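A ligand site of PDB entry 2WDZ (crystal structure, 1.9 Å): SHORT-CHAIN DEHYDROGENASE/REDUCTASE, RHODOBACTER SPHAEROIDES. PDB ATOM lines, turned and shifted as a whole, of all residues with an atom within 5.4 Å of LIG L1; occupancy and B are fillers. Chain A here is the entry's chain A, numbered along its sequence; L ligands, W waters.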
ATOM      1  N   GLY A  18       5.389 -13.285  -7.679  1.00  0.00           N
ATOM      2  CA  GLY A  18       4.925 -12.514  -8.821  1.00  0.00           C
ATOM      3  C   GLY A  18       4.942 -13.270 -10.109  1.00  0.00           C
ATOM      4  O   GLY A  18       5.090 -12.670 -11.184  1.00  0.00           O
ATOM      5  N   ALA A  19       4.787 -14.597 -10.015  1.00  0.00           N
ATOM      6  CA  ALA A  19       4.978 -15.488 -11.129  1.00  0.00           C
ATOM      7  C   ALA A  19       3.844 -15.314 -12.136  1.00  0.00           C
ATOM      8  O   ALA A  19       4.028 -15.625 -13.308  1.00  0.00           O
ATOM      9  CB  ALA A  19       5.073 -16.902 -10.669  1.00  0.00           C
ATOM     10  N   GLY A  20       2.727 -14.736 -11.672  1.00  0.00           N
ATOM     11  CA  GLY A  20       1.512 -14.658 -12.457  1.00  0.00           C
ATOM     12  C   GLY A  20       1.521 -13.652 -13.604  1.00  0.00           C
ATOM     13  O   GLY A  20       0.705 -13.736 -14.524  1.00  0.00           O
ATOM     14  N   SER A  21       2.430 -12.692 -13.577  1.00  0.00           N
ATOM     15  CA  SER A  21       2.363 -11.629 -14.561  1.00  0.00           C
ATOM     16  C   SER A  21       3.745 -11.047 -14.883  1.00  0.00           C
ATOM     17  O   SER A  21       4.722 -11.230 -14.123  1.00  0.00           O
ATOM     18  CB  SER A  21       1.346 -10.536 -14.097  1.00  0.00           C
ATOM     19  OG  SER A  21       1.715  -9.202 -14.409  1.00  0.00           O
ATOM     20  N   GLY A  22       3.812 -10.356 -16.019  1.00  0.00           N
ATOM     21  CA  GLY A  22       4.973  -9.539 -16.378  1.00  0.00           C
ATOM     22  C   GLY A  22       6.325 -10.207 -16.197  1.00  0.00           C
ATOM     23  O   GLY A  22       6.623 -11.274 -16.784  1.00  0.00           O
ATOM     24  N   ILE A  23       7.207  -9.553 -15.476  1.00  0.00           N
ATOM     25  CA  ILE A  23       8.576  -9.954 -15.447  1.00  0.00           C
ATOM     26  C   ILE A  23       8.743 -11.293 -14.696  1.00  0.00           C
ATOM     27  O   ILE A  23       9.492 -12.094 -15.087  1.00  0.00           O
ATOM     28  CB  ILE A  23       9.438  -8.875 -14.809  1.00  0.00           C
ATOM     29  CG1 ILE A  23       9.480  -7.632 -15.667  1.00  0.00           C
ATOM     30  CG2 ILE A  23      10.808  -9.377 -14.481  1.00  0.00           C
ATOM     31  CD1 ILE A  23      10.272  -6.590 -15.115  1.00  0.00           C
ATOM     32  N   GLY A  24       7.974 -11.484 -13.645  1.00  0.00           N
ATOM     33  CA  GLY A  24       7.982 -12.748 -12.843  1.00  0.00           C
ATOM     34  C   GLY A  24       7.654 -13.961 -13.725  1.00  0.00           C
ATOM     35  O   GLY A  24       8.396 -14.963 -13.747  1.00  0.00           O
ATOM     36  N   ILE A  41       4.442 -18.512  -7.124  1.00  0.00           N
ATOM     37  CA  ILE A  41       3.800 -17.818  -6.026  1.00  0.00           C
ATOM     38  C   ILE A  41       3.248 -16.493  -6.480  1.00  0.00           C
ATOM     39  O   ILE A  41       3.992 -15.643  -6.957  1.00  0.00           O
ATOM     40  CB  ILE A  41       4.800 -17.621  -4.868  1.00  0.00           C
ATOM     41  CG1 ILE A  41       5.452 -18.964  -4.509  1.00  0.00           C
ATOM     42  CG2 ILE A  41       4.127 -16.986  -3.652  1.00  0.00           C
ATOM     43  N   ASP A  42       1.939 -16.302  -6.264  1.00  0.00           N
ATOM     44  CA  ASP A  42       1.252 -15.054  -6.557  1.00  0.00           C
ATOM     45  C   ASP A  42       0.010 -14.962  -5.682  1.00  0.00           C
ATOM     46  O   ASP A  42      -0.611 -15.981  -5.383  1.00  0.00           O
ATOM     47  CB  ASP A  42       0.853 -14.999  -8.022  1.00  0.00           C
ATOM     48  CG  ASP A  42       0.857 -13.586  -8.566  1.00  0.00           C
ATOM     49  OD1 ASP A  42      -0.026 -12.765  -8.184  1.00  0.00           O
ATOM     50  OD2 ASP A  42       1.760 -13.288  -9.387  1.00  0.00           O
ATOM     51  N   ARG A  43      -0.384 -13.735  -5.286  1.00  0.00           N
ATOM     52  CA  ARG A  43      -1.681 -13.582  -4.618  1.00  0.00           C
ATOM     53  C   ARG A  43      -2.857 -13.778  -5.570  1.00  0.00           C
ATOM     54  O   ARG A  43      -3.957 -14.043  -5.125  1.00  0.00           O
ATOM     55  CB  ARG A  43      -1.767 -12.268  -3.826  1.00  0.00           C
ATOM     56  CG  ARG A  43      -1.864 -10.949  -4.618  1.00  0.00           C
ATOM     57  CD  ARG A  43      -2.393  -9.790  -3.729  1.00  0.00           C
ATOM     58  NE  ARG A  43      -1.939  -8.468  -4.179  1.00  0.00           N
ATOM     59  CZ  ARG A  43      -1.546  -7.450  -3.385  1.00  0.00           C
ATOM     60  NH1 ARG A  43      -1.537  -7.568  -2.056  1.00  0.00           N
ATOM     61  NH2 ARG A  43      -1.134  -6.300  -3.922  1.00  0.00           N
ATOM     62  N   GLU A  44      -2.642 -13.660  -6.864  1.00  0.00           N
ATOM     63  CA  GLU A  44      -3.727 -13.849  -7.843  1.00  0.00           C
ATOM     64  C   GLU A  44      -3.821 -15.281  -8.347  1.00  0.00           C
ATOM     65  O   GLU A  44      -3.032 -15.714  -9.191  1.00  0.00           O
ATOM     66  CB  GLU A  44      -3.634 -12.856  -9.024  1.00  0.00           C
ATOM     67  CG  GLU A  44      -4.808 -13.003 -10.046  1.00  0.00           C
ATOM     68  CD  GLU A  44      -4.804 -12.000 -11.205  1.00  0.00           C
ATOM     69  OE1 GLU A  44      -5.531 -12.298 -12.203  1.00  0.00           O
ATOM     70  OE2 GLU A  44      -4.087 -10.933 -11.121  1.00  0.00           O
ATOM     71  N   ALA A  47      -4.193 -15.726 -12.275  1.00  0.00           N
ATOM     72  CA  ALA A  47      -2.912 -15.532 -12.966  1.00  0.00           C
ATOM     73  C   ALA A  47      -1.993 -16.735 -12.789  1.00  0.00           C
ATOM     74  O   ALA A  47      -1.346 -17.160 -13.731  1.00  0.00           O
ATOM     75  CB  ALA A  47      -2.237 -14.288 -12.440  1.00  0.00           C
ATOM     76  N   ALA A  65      -0.499 -17.051  -2.429  1.00  0.00           N
ATOM     77  CA  ALA A  65       0.009 -16.451  -1.199  1.00  0.00           C
ATOM     78  C   ALA A  65       0.228 -14.958  -1.406  1.00  0.00           C
ATOM     79  O   ALA A  65       0.640 -14.522  -2.491  1.00  0.00           O
ATOM     80  CB  ALA A  65       1.304 -17.123  -0.752  1.00  0.00           C
ATOM     81  N   ASP A  66      -0.101 -14.195  -0.371  1.00  0.00           N
ATOM     82  CA  ASP A  66       0.201 -12.775  -0.285  1.00  0.00           C
ATOM     83  C   ASP A  66       1.567 -12.667   0.359  1.00  0.00           C
ATOM     84  O   ASP A  66       1.730 -13.105   1.498  1.00  0.00           O
ATOM     85  CB  ASP A  66      -0.816 -12.071   0.644  1.00  0.00           C
ATOM     86  CG  ASP A  66      -0.801 -10.544   0.527  1.00  0.00           C
ATOM     87  OD1 ASP A  66       0.254  -9.898   0.270  1.00  0.00           O
ATOM     88  OD2 ASP A  66      -1.895  -9.983   0.738  1.00  0.00           O
ATOM     89  N   VAL A  67       2.542 -12.091  -0.354  1.00  0.00           N
ATOM     90  CA  VAL A  67       3.862 -11.940   0.194  1.00  0.00           C
ATOM     91  C   VAL A  67       3.909 -11.051   1.449  1.00  0.00           C
ATOM     92  O   VAL A  67       4.852 -11.186   2.228  1.00  0.00           O
ATOM     93  CB  VAL A  67       4.935 -11.478  -0.859  1.00  0.00           C
ATOM     94  CG1 VAL A  67       4.933 -12.417  -2.113  1.00  0.00           C
ATOM     95  CG2 VAL A  67       4.751 -10.026  -1.234  1.00  0.00           C
ATOM     96  N   THR A  68       2.938 -10.158   1.659  1.00  0.00           N
ATOM     97  CA  THR A  68       2.971  -9.317   2.877  1.00  0.00           C
ATOM     98  C   THR A  68       2.662 -10.062   4.192  1.00  0.00           C
ATOM     99  O   THR A  68       2.989  -9.581   5.296  1.00  0.00           O
ATOM    100  CB  THR A  68       2.033  -8.092   2.791  1.00  0.00           C
ATOM    101  OG1 THR A  68       0.679  -8.536   2.848  1.00  0.00           O
ATOM    102  CG2 THR A  68       2.279  -7.296   1.507  1.00  0.00           C
ATOM    103  N   ASN A  91      12.334 -12.691  -6.046  1.00  0.00           N
ATOM    104  CA  ASN A  91      11.339 -11.815  -5.413  1.00  0.00           C
ATOM    105  C   ASN A  91      10.878 -10.812  -6.452  1.00  0.00           C
ATOM    106  O   ASN A  91      11.491  -9.761  -6.589  1.00  0.00           O
ATOM    107  CB  ASN A  91      11.990 -11.079  -4.221  1.00  0.00           C
ATOM    108  CG  ASN A  91      12.175 -11.975  -3.039  1.00  0.00           C
ATOM    109  OD1 ASN A  91      13.275 -12.071  -2.452  1.00  0.00           O
ATOM    110  ND2 ASN A  91      11.129 -12.664  -2.686  1.00  0.00           N
ATOM    111  N   SER A  92       9.848 -11.161  -7.205  1.00  0.00           N
ATOM    112  CA  SER A  92       9.327 -10.319  -8.292  1.00  0.00           C
ATOM    113  C   SER A  92       7.978  -9.632  -7.929  1.00  0.00           C
ATOM    114  O   SER A  92       7.698  -8.566  -8.467  1.00  0.00           O
ATOM    115  CB  SER A  92       9.282 -11.059  -9.637  1.00  0.00           C
ATOM    116  OG  SER A  92       8.868 -10.143 -10.673  1.00  0.00           O
ATOM    117  N   ALA A  93       7.213 -10.192  -6.980  1.00  0.00           N
ATOM    118  CA  ALA A  93       5.969  -9.580  -6.459  1.00  0.00           C
ATOM    119  C   ALA A  93       6.206  -8.113  -6.109  1.00  0.00           C
ATOM    120  O   ALA A  93       7.065  -7.808  -5.260  1.00  0.00           O
ATOM    121  CB  ALA A  93       5.460 -10.331  -5.205  1.00  0.00           C
ATOM    122  N   GLY A  94       5.455  -7.205  -6.736  1.00  0.00           N
ATOM    123  CA  GLY A  94       5.631  -5.806  -6.412  1.00  0.00           C
ATOM    124  C   GLY A  94       4.547  -4.939  -7.014  1.00  0.00           C
ATOM    125  O   GLY A  94       3.885  -5.368  -7.966  1.00  0.00           O
ATOM    126  N   ILE A  95       4.339  -3.691  -6.596  1.00  0.00           N
ATOM    127  CA  ILE A  95       3.375  -2.691  -7.041  1.00  0.00           C
ATOM    128  C   ILE A  95       3.928  -1.272  -7.178  1.00  0.00           C
ATOM    129  O   ILE A  95       4.896  -0.878  -6.506  1.00  0.00           O
ATOM    130  CB  ILE A  95       2.181  -2.670  -6.064  1.00  0.00           C
ATOM    131  CG1 ILE A  95       2.649  -2.297  -4.651  1.00  0.00           C
ATOM    132  CG2 ILE A  95       1.476  -4.018  -6.061  1.00  0.00           C
ATOM    133  CD1 ILE A  95       1.518  -2.050  -3.683  1.00  0.00           C
ATOM    134  N   VAL A 115       4.390  -4.458   0.278  1.00  0.00           N
ATOM    135  CA  VAL A 115       4.607  -5.455  -0.754  1.00  0.00           C
ATOM    136  C   VAL A 115       6.048  -5.437  -1.214  1.00  0.00           C
ATOM    137  O   VAL A 115       6.727  -6.472  -1.222  1.00  0.00           O
ATOM    138  CB  VAL A 115       3.709  -5.260  -2.017  1.00  0.00           C
ATOM    139  CG1 VAL A 115       4.092  -6.280  -3.070  1.00  0.00           C
ATOM    140  CG2 VAL A 115       2.259  -5.396  -1.633  1.00  0.00           C
ATOM    141  N   ASN A 116       6.495  -4.255  -1.623  1.00  0.00           N
ATOM    142  CA  ASN A 116       7.805  -4.135  -2.227  1.00  0.00           C
ATOM    143  C   ASN A 116       8.994  -4.432  -1.339  1.00  0.00           C
ATOM    144  O   ASN A 116      10.014  -4.885  -1.825  1.00  0.00           O
ATOM    145  CB  ASN A 116       7.981  -2.740  -2.867  1.00  0.00           C
ATOM    146  CG  ASN A 116       7.012  -2.530  -4.030  1.00  0.00           C
ATOM    147  OD1 ASN A 116       6.182  -3.357  -4.280  1.00  0.00           O
ATOM    148  ND2 ASN A 116       7.130  -1.388  -4.712  1.00  0.00           N
ATOM    149  N   LEU A 142      13.949  -8.130  -7.478  1.00  0.00           N
ATOM    150  CA  LEU A 142      13.563  -7.070  -8.407  1.00  0.00           C
ATOM    151  C   LEU A 142      13.617  -5.676  -7.762  1.00  0.00           C
ATOM    152  O   LEU A 142      12.688  -5.247  -7.086  1.00  0.00           O
ATOM    153  CB  LEU A 142      12.281  -7.383  -9.175  1.00  0.00           C
ATOM    154  CG  LEU A 142      12.928  -8.135 -10.348  1.00  0.00           C
ATOM    155  CD1 LEU A 142      12.780  -9.602 -10.211  1.00  0.00           C
ATOM    156  CD2 LEU A 142      12.743  -7.565 -11.760  1.00  0.00           C
ATOM    157  N   GLY A 143      14.773  -5.042  -7.934  1.00  0.00           N
ATOM    158  CA  GLY A 143      14.977  -3.646  -7.605  1.00  0.00           C
ATOM    159  C   GLY A 143      14.430  -2.817  -8.725  1.00  0.00           C
ATOM    160  O   GLY A 143      13.521  -3.205  -9.354  1.00  0.00           O
ATOM    161  N   SER A 144      15.000  -1.654  -8.969  1.00  0.00           N
ATOM    162  CA  SER A 144      14.481  -0.763 -10.039  1.00  0.00           C
ATOM    163  C   SER A 144      15.551   0.309 -10.274  1.00  0.00           C
ATOM    164  O   SER A 144      16.302   0.659  -9.349  1.00  0.00           O
ATOM    165  CB  SER A 144      13.175  -0.114  -9.605  1.00  0.00           C
ATOM    166  OG  SER A 144      12.604   0.704 -10.624  1.00  0.00           O
ATOM    167  N   MET A 145      15.557   0.893 -11.465  1.00  0.00           N
ATOM    168  CA  MET A 145      16.252   2.157 -11.608  1.00  0.00           C
ATOM    169  C   MET A 145      15.734   3.141 -10.540  1.00  0.00           C
ATOM    170  O   MET A 145      16.479   4.021 -10.123  1.00  0.00           O
ATOM    171  CB  MET A 145      16.154   2.692 -13.042  1.00  0.00           C
ATOM    172  CG  MET A 145      14.892   3.428 -13.338  1.00  0.00           C
ATOM    173  SD  MET A 145      14.995   3.858 -15.073  1.00  0.00           S
ATOM    174  CE  MET A 145      13.419   4.669 -15.336  1.00  0.00           C
ATOM    175  N   TYR A 159       7.439   4.520  -3.975  1.00  0.00           N
ATOM    176  CA  TYR A 159       8.039   3.521  -4.884  1.00  0.00           C
ATOM    177  C   TYR A 159       9.530   3.727  -4.882  1.00  0.00           C
ATOM    178  O   TYR A 159      10.295   2.759  -4.796  1.00  0.00           O
ATOM    179  CB  TYR A 159       7.501   3.657  -6.324  1.00  0.00           C
ATOM    180  CG  TYR A 159       7.966   2.550  -7.270  1.00  0.00           C
ATOM    181  CD1 TYR A 159       7.356   1.277  -7.219  1.00  0.00           C
ATOM    182  CD2 TYR A 159       8.981   2.770  -8.225  1.00  0.00           C
ATOM    183  CE1 TYR A 159       7.751   0.234  -8.048  1.00  0.00           C
ATOM    184  CE2 TYR A 159       9.415   1.736  -9.065  1.00  0.00           C
ATOM    185  CZ  TYR A 159       8.773   0.458  -8.990  1.00  0.00           C
ATOM    186  OH  TYR A 159       9.143  -0.533  -9.806  1.00  0.00           O
ATOM    187  N   LYS A 163      12.224   0.934  -3.323  1.00  0.00           N
ATOM    188  CA  LYS A 163      13.333   0.441  -4.134  1.00  0.00           C
ATOM    189  C   LYS A 163      14.684   0.753  -3.571  1.00  0.00           C
ATOM    190  O   LYS A 163      15.632  -0.065  -3.679  1.00  0.00           O
ATOM    191  CB  LYS A 163      13.166   0.853  -5.583  1.00  0.00           C
ATOM    192  CG  LYS A 163      11.905   0.175  -6.199  1.00  0.00           C
ATOM    193  CD  LYS A 163      11.943  -1.333  -6.127  1.00  0.00           C
ATOM    194  CE  LYS A 163      10.742  -1.898  -6.817  1.00  0.00           C
ATOM    195  NZ  LYS A 163      10.577  -3.412  -6.788  1.00  0.00           N
ATOM    196  N   PRO A 189      15.876  -2.725 -13.311  1.00  0.00           N
ATOM    197  CA  PRO A 189      15.361  -2.473 -14.672  1.00  0.00           C
ATOM    198  C   PRO A 189      14.973  -1.004 -14.880  1.00  0.00           C
ATOM    199  O   PRO A 189      14.547  -0.320 -13.924  1.00  0.00           O
ATOM    200  CB  PRO A 189      14.102  -3.357 -14.754  1.00  0.00           C
ATOM    201  CG  PRO A 189      14.092  -4.240 -13.609  1.00  0.00           C
ATOM    202  CD  PRO A 189      15.004  -3.663 -12.538  1.00  0.00           C
ATOM    203  N   GLY A 190      15.087  -0.555 -16.123  1.00  0.00           N
ATOM    204  CA  GLY A 190      14.399   0.670 -16.609  1.00  0.00           C
ATOM    205  C   GLY A 190      12.934   0.402 -16.869  1.00  0.00           C
ATOM    206  O   GLY A 190      12.368  -0.543 -16.311  1.00  0.00           O
ATOM    207  N   TYR A 191      12.281   1.231 -17.678  1.00  0.00           N
ATOM    208  CA  TYR A 191      10.904   0.929 -18.065  1.00  0.00           C
ATOM    209  C   TYR A 191      10.910  -0.404 -18.864  1.00  0.00           C
ATOM    210  O   TYR A 191      11.798  -0.638 -19.694  1.00  0.00           O
ATOM    211  CB  TYR A 191      10.253   2.112 -18.819  1.00  0.00           C
ATOM    212  CG  TYR A 191      10.231   3.409 -17.987  1.00  0.00           C
ATOM    213  CD1 TYR A 191       9.395   3.541 -16.873  1.00  0.00           C
ATOM    214  CD2 TYR A 191      11.050   4.489 -18.320  1.00  0.00           C
ATOM    215  CE1 TYR A 191       9.367   4.733 -16.082  1.00  0.00           C
ATOM    216  CE2 TYR A 191      11.059   5.677 -17.575  1.00  0.00           C
ATOM    217  CZ  TYR A 191      10.223   5.788 -16.432  1.00  0.00           C
ATOM    218  OH  TYR A 191      10.231   6.952 -15.705  1.00  0.00           O
ATOM    219  N   VAL A 192       9.987  -1.287 -18.514  1.00  0.00           N
ATOM    220  CA  VAL A 192       9.747  -2.582 -19.141  1.00  0.00           C
ATOM    221  C   VAL A 192       8.263  -2.601 -19.564  1.00  0.00           C
ATOM    222  O   VAL A 192       7.379  -2.206 -18.788  1.00  0.00           O
ATOM    223  CB  VAL A 192      10.064  -3.754 -18.176  1.00  0.00           C
ATOM    224  CG1 VAL A 192       9.998  -5.117 -18.863  1.00  0.00           C
ATOM    225  CG2 VAL A 192      11.443  -3.570 -17.520  1.00  0.00           C
ATOM    226  N   THR A 194       5.244  -3.984 -19.424  1.00  0.00           N
ATOM    227  CA  THR A 194       4.410  -4.978 -18.709  1.00  0.00           C
ATOM    228  C   THR A 194       3.043  -4.380 -18.289  1.00  0.00           C
ATOM    229  O   THR A 194       2.722  -3.250 -18.659  1.00  0.00           O
ATOM    230  CB  THR A 194       5.096  -5.565 -17.429  1.00  0.00           C
ATOM    231  OG1 THR A 194       5.253  -4.526 -16.455  1.00  0.00           O
ATOM    232  CG2 THR A 194       6.425  -6.246 -17.713  1.00  0.00           C
ATOM    233  N   GLU A 195       2.261  -5.155 -17.521  1.00  0.00           N
ATOM    234  CA  GLU A 195       1.002  -4.726 -16.897  1.00  0.00           C
ATOM    235  C   GLU A 195       1.145  -3.534 -15.951  1.00  0.00           C
ATOM    236  O   GLU A 195       0.265  -2.653 -15.914  1.00  0.00           O
ATOM    237  CB  GLU A 195       0.363  -5.894 -16.126  1.00  0.00           C
ATOM    238  CG  GLU A 195      -0.773  -6.573 -16.846  1.00  0.00           C
ATOM    239  CD  GLU A 195      -1.971  -5.631 -17.034  1.00  0.00           C
ATOM    240  OE1 GLU A 195      -2.272  -5.232 -18.189  1.00  0.00           O
ATOM    241  OE2 GLU A 195      -2.587  -5.264 -16.011  1.00  0.00           O
ATOM    242  N   MET A 196       2.223  -3.531 -15.158  1.00  0.00           N
ATOM    243  CA  MET A 196       2.555  -2.458 -14.217  1.00  0.00           C
ATOM    244  C   MET A 196       2.761  -1.099 -14.892  1.00  0.00           C
ATOM    245  O   MET A 196       2.656  -0.037 -14.246  1.00  0.00           O
ATOM    246  CB  MET A 196       3.830  -2.805 -13.449  1.00  0.00           C
ATOM    247  CG  MET A 196       4.226  -1.706 -12.439  1.00  0.00           C
ATOM    248  SD  MET A 196       5.619  -2.110 -11.366  1.00  0.00           S
ATOM    249  CE  MET A 196       4.905  -3.391 -10.332  1.00  0.00           C
ATOM    250  N   THR A 197       3.102  -1.126 -16.171  1.00  0.00           N
ATOM    251  CA  THR A 197       3.391   0.101 -16.921  1.00  0.00           C
ATOM    252  C   THR A 197       2.458   0.307 -18.131  1.00  0.00           C
ATOM    253  O   THR A 197       2.745   1.121 -19.022  1.00  0.00           O
ATOM    254  CB  THR A 197       4.893   0.162 -17.372  1.00  0.00           C
ATOM    255  OG1 THR A 197       5.215  -1.022 -18.106  1.00  0.00           O
ATOM    256  CG2 THR A 197       5.819   0.309 -16.143  1.00  0.00           C
HETATM  257  P1  LIG L   1       3.381  -6.922 -12.716  1.00  0.00           P
HETATM  258  O1  LIG L   1       3.251  -7.282 -14.164  1.00  0.00           O
HETATM  259  O2  LIG L   1       2.428  -6.030 -12.019  1.00  0.00           O
HETATM  260  O3  LIG L   1       3.490  -8.312 -11.909  1.00  0.00           O
HETATM  261  C1  LIG L   1       3.439  -8.256 -10.481  1.00  0.00           C
HETATM  262  C2  LIG L   1       2.999  -9.612  -9.964  1.00  0.00           C
HETATM  263  O4  LIG L   1       3.161  -9.588  -8.543  1.00  0.00           O
HETATM  264  C3  LIG L   1       1.502  -9.737 -10.288  1.00  0.00           C
HETATM  265  O5  LIG L   1       1.305 -11.054 -10.833  1.00  0.00           O
HETATM  266  C4  LIG L   1       0.795  -9.531  -8.933  1.00  0.00           C
HETATM  267  O6  LIG L   1      -0.362 -10.350  -8.831  1.00  0.00           O
HETATM  268  C5  LIG L   1       1.914 -10.023  -7.961  1.00  0.00           C
HETATM  269  N1  LIG L   1       1.724  -9.487  -6.552  1.00  0.00           N
HETATM  270  C6  LIG L   1       1.452  -8.204  -6.203  1.00  0.00           C
HETATM  271  N2  LIG L   1       1.328  -8.094  -4.867  1.00  0.00           N
HETATM  272  C7  LIG L   1       1.511  -9.329  -4.384  1.00  0.00           C
HETATM  273  C8  LIG L   1       1.492  -9.872  -3.079  1.00  0.00           C
HETATM  274  N3  LIG L   1       1.277  -9.080  -2.015  1.00  0.00           N
HETATM  275  N4  LIG L   1       1.726 -11.196  -2.937  1.00  0.00           N
HETATM  276  C9  LIG L   1       1.989 -12.001  -3.946  1.00  0.00           C
HETATM  277  N5  LIG L   1       1.992 -11.548  -5.212  1.00  0.00           N
HETATM  278  C10 LIG L   1       1.760 -10.215  -5.453  1.00  0.00           C
HETATM  279  O7  LIG L   1       4.923  -6.239 -12.419  1.00  0.00           O
HETATM  280  P2  LIG L   1       6.388  -6.496 -13.182  1.00  0.00           P
HETATM  281  O8  LIG L   1       6.145  -7.925 -13.517  1.00  0.00           O
HETATM  282  O9  LIG L   1       6.094  -5.315 -14.057  1.00  0.00           O
HETATM  283  O10 LIG L   1       7.167  -6.116 -11.815  1.00  0.00           O
HETATM  284  C11 LIG L   1       7.774  -7.080 -10.987  1.00  0.00           C
HETATM  285  C12 LIG L   1       8.911  -6.435 -10.203  1.00  0.00           C
HETATM  286  O11 LIG L   1       9.811  -5.721 -11.128  1.00  0.00           O
HETATM  287  C13 LIG L   1       8.294  -5.401  -9.257  1.00  0.00           C
HETATM  288  O12 LIG L   1       9.029  -5.393  -8.056  1.00  0.00           O
HETATM  289  C14 LIG L   1       8.533  -4.079  -9.985  1.00  0.00           C
HETATM  290  O13 LIG L   1       8.513  -2.996  -9.040  1.00  0.00           O
HETATM  291  C15 LIG L   1       9.908  -4.339 -10.675  1.00  0.00           C
HETATM  292  N6  LIG L   1      10.173  -3.406 -11.805  1.00  0.00           N
HETATM  293  C16 LIG L   1       9.255  -3.235 -12.948  1.00  0.00           C
HETATM  294  C17 LIG L   1       9.593  -2.315 -13.956  1.00  0.00           C
HETATM  295  C18 LIG L   1       8.617  -2.146 -15.096  1.00  0.00           C
HETATM  296  O14 LIG L   1       7.743  -3.161 -15.340  1.00  0.00           O
HETATM  297  N7  LIG L   1       8.621  -0.991 -15.778  1.00  0.00           N
HETATM  298  C19 LIG L   1      10.772  -1.558 -13.867  1.00  0.00           C
HETATM  299  C20 LIG L   1      11.610  -1.745 -12.772  1.00  0.00           C
HETATM  300  C21 LIG L   1      11.344  -2.672 -11.771  1.00  0.00           C
HETATM  301  C1  LG2 L   2       7.568   2.314 -11.946  1.00  0.00           C
HETATM  302  O1  LG2 L   2       8.304   1.355 -14.020  1.00  0.00           O
HETATM  303  C2  LG2 L   2       6.348   3.246 -12.050  1.00  0.00           C
HETATM  304  C3  LG2 L   2      10.016   2.574 -12.731  1.00  0.00           C
HETATM  305  O2  LG2 L   2      10.677   1.309 -12.517  1.00  0.00           O
HETATM  306  C4  LG2 L   2       6.705   4.694 -11.692  1.00  0.00           C
HETATM  307  C5  LG2 L   2       8.519   2.458 -13.137  1.00  0.00           C
HETATM  308  O   HOH W   1       9.913  -7.308  -6.178  1.00  0.00           O
HETATM  309  O   HOH W   2      -0.373  -6.009 -12.740  1.00  0.00           O
HETATM  310  O   HOH W   3       1.774  -4.780  -9.940  1.00  0.00           O
HETATM  311  O   HOH W   4       6.169  -9.970 -11.800  1.00  0.00           O
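Residues that only touch LIG L1: Gly 190 (3.1 Å), Thr 197 (3.1 Å), Ala 65 (3.2 Å), Gly 143 (3.3 Å), Ser 144 (3.4 Å), Gly 18 (3.4 Å), Met 196 (3.4 Å), Pro 189 (3.5 Å), Gly 22 (3.5 Å), Ala 93 (3.5 Å), Leu 142 (3.5 Å), Glu 195 (3.8 Å), Tyr 191 (3.8 Å), Val 115 (3.8 Å), Gly 94 (3.8 Å) and Gly 20 (3.8 Å).
Hydrophobic or aromatic side chains that line LIG L1: Ile 23, Val 67, Ala 93, Val 115, Leu 142, Tyr 159, Pro 189, Val 192 and Met 196.
Of the 37 residues printed, 27 come within 4 Å of LIG L1.
The nearest printed residue that does not touch LIG L1 is Gly 24 (4.004 Å).
A nitrogen (N7) of LIG L1 is in hydrogen-bond range of an oxygen (O1) of LG2 L2 (2.9 Å).
The side-chain hydroxyl of Thr 197 is in hydrogen-bond range of the backbone NH of Thr 194 (3.2 Å).
The backbone NH (N) of Glu 44 sits at hydrogen-bond distance from the side-chain carboxylate (OD1) of Asp 42 (3.1 Å).
The backbone carbonyl oxygen of Ile 41 sits at hydrogen-bond distance from the backbone NH of Gly 18, 2.8 Å away.
The side-chain carboxylate of Asp 42 lies within hydrogen-bond range of the backbone NH of Ala 19 (3.4 Å).
O of Val 192 is in hydrogen-bond range of OG1 of Thr 197 (2.6 Å).
The side-chain carboxylate of Asp 66 lies within salt-bridge range of the guanidinium group of Arg 43, 3.7 Å away.
The side-chain carboxylate (OD2) of Asp 42 lies within hydrogen-bond range of the backbone NH (N) of Gly 20, at 2.9 Å.
OG1 of Thr 68 sits at hydrogen-bond distance from OD1 of Asp 66, at 2.9 Å.
N4 of LIG L1 is in hydrogen-bond range of N of Val 67 (2.9 Å).
The backbone carbonyl oxygen (O) of Ser 92 lies close to an oxygen (O12) of LIG L1 (3.5 Å).
The side-chain hydroxyl of Ser 21 sits at hydrogen-bond distance from an oxygen (O1) of LIG L1.
O8 of LIG L1 sits at hydrogen-bond distance from N of Ile 23, 2.8 Å away.
An oxygen (O9) of LIG L1 sits at hydrogen-bond distance from the side-chain hydroxyl of Thr 194, at 2.7 Å.
O2 of LG2 L2 lies within hydrogen-bond range of OG of Ser 144, at 2.8 Å.
The side-chain carboxylate (OD1) of Asp 66 sits at hydrogen-bond distance from a nitrogen (N3) of LIG L1 (2.6 Å).
A nitrogen (N7) of LIG L1 is in hydrogen-bond range of the backbone carbonyl oxygen (O) of Val 192, 3.5 Å away.
The backbone NH of Ser 21 lies close to an oxygen (O5) of LIG L1 (3.4 Å).
An oxygen (O13) of LIG L1 lies within hydrogen-bond range of the side-chain hydroxyl (OH) of Tyr 159, 2.7 Å away.
The side-chain amino group of Lys 163 sits at hydrogen-bond distance from an oxygen (O12) of LIG L1.
An oxygen (O6) of LIG L1 sits at hydrogen-bond distance from the side-chain carboxylate (OD1) of Asp 42.
NH2 of Arg 43 is in hydrogen-bond range of N2 of LIG L1.
N of Arg 43 lies close to N5 of LIG L1 (3.2 Å).
Water W3 bridges an oxygen (O2) of LIG L1 (2.5 Å) and the backbone carbonyl oxygen of Gly 94 (2.9 Å).
Water W4 lies within hydrogen-bond range of an oxygen (O8) of LIG L1 (2.7 Å), the side-chain hydroxyl (OG) of Ser 92 (2.9 Å), the backbone carbonyl oxygen (O) of Gly 18 (3.0 Å), the backbone NH (N) of Gly 24 (3.0 Å) and the backbone carbonyl oxygen (O) of Ser 21 (3.0 Å).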
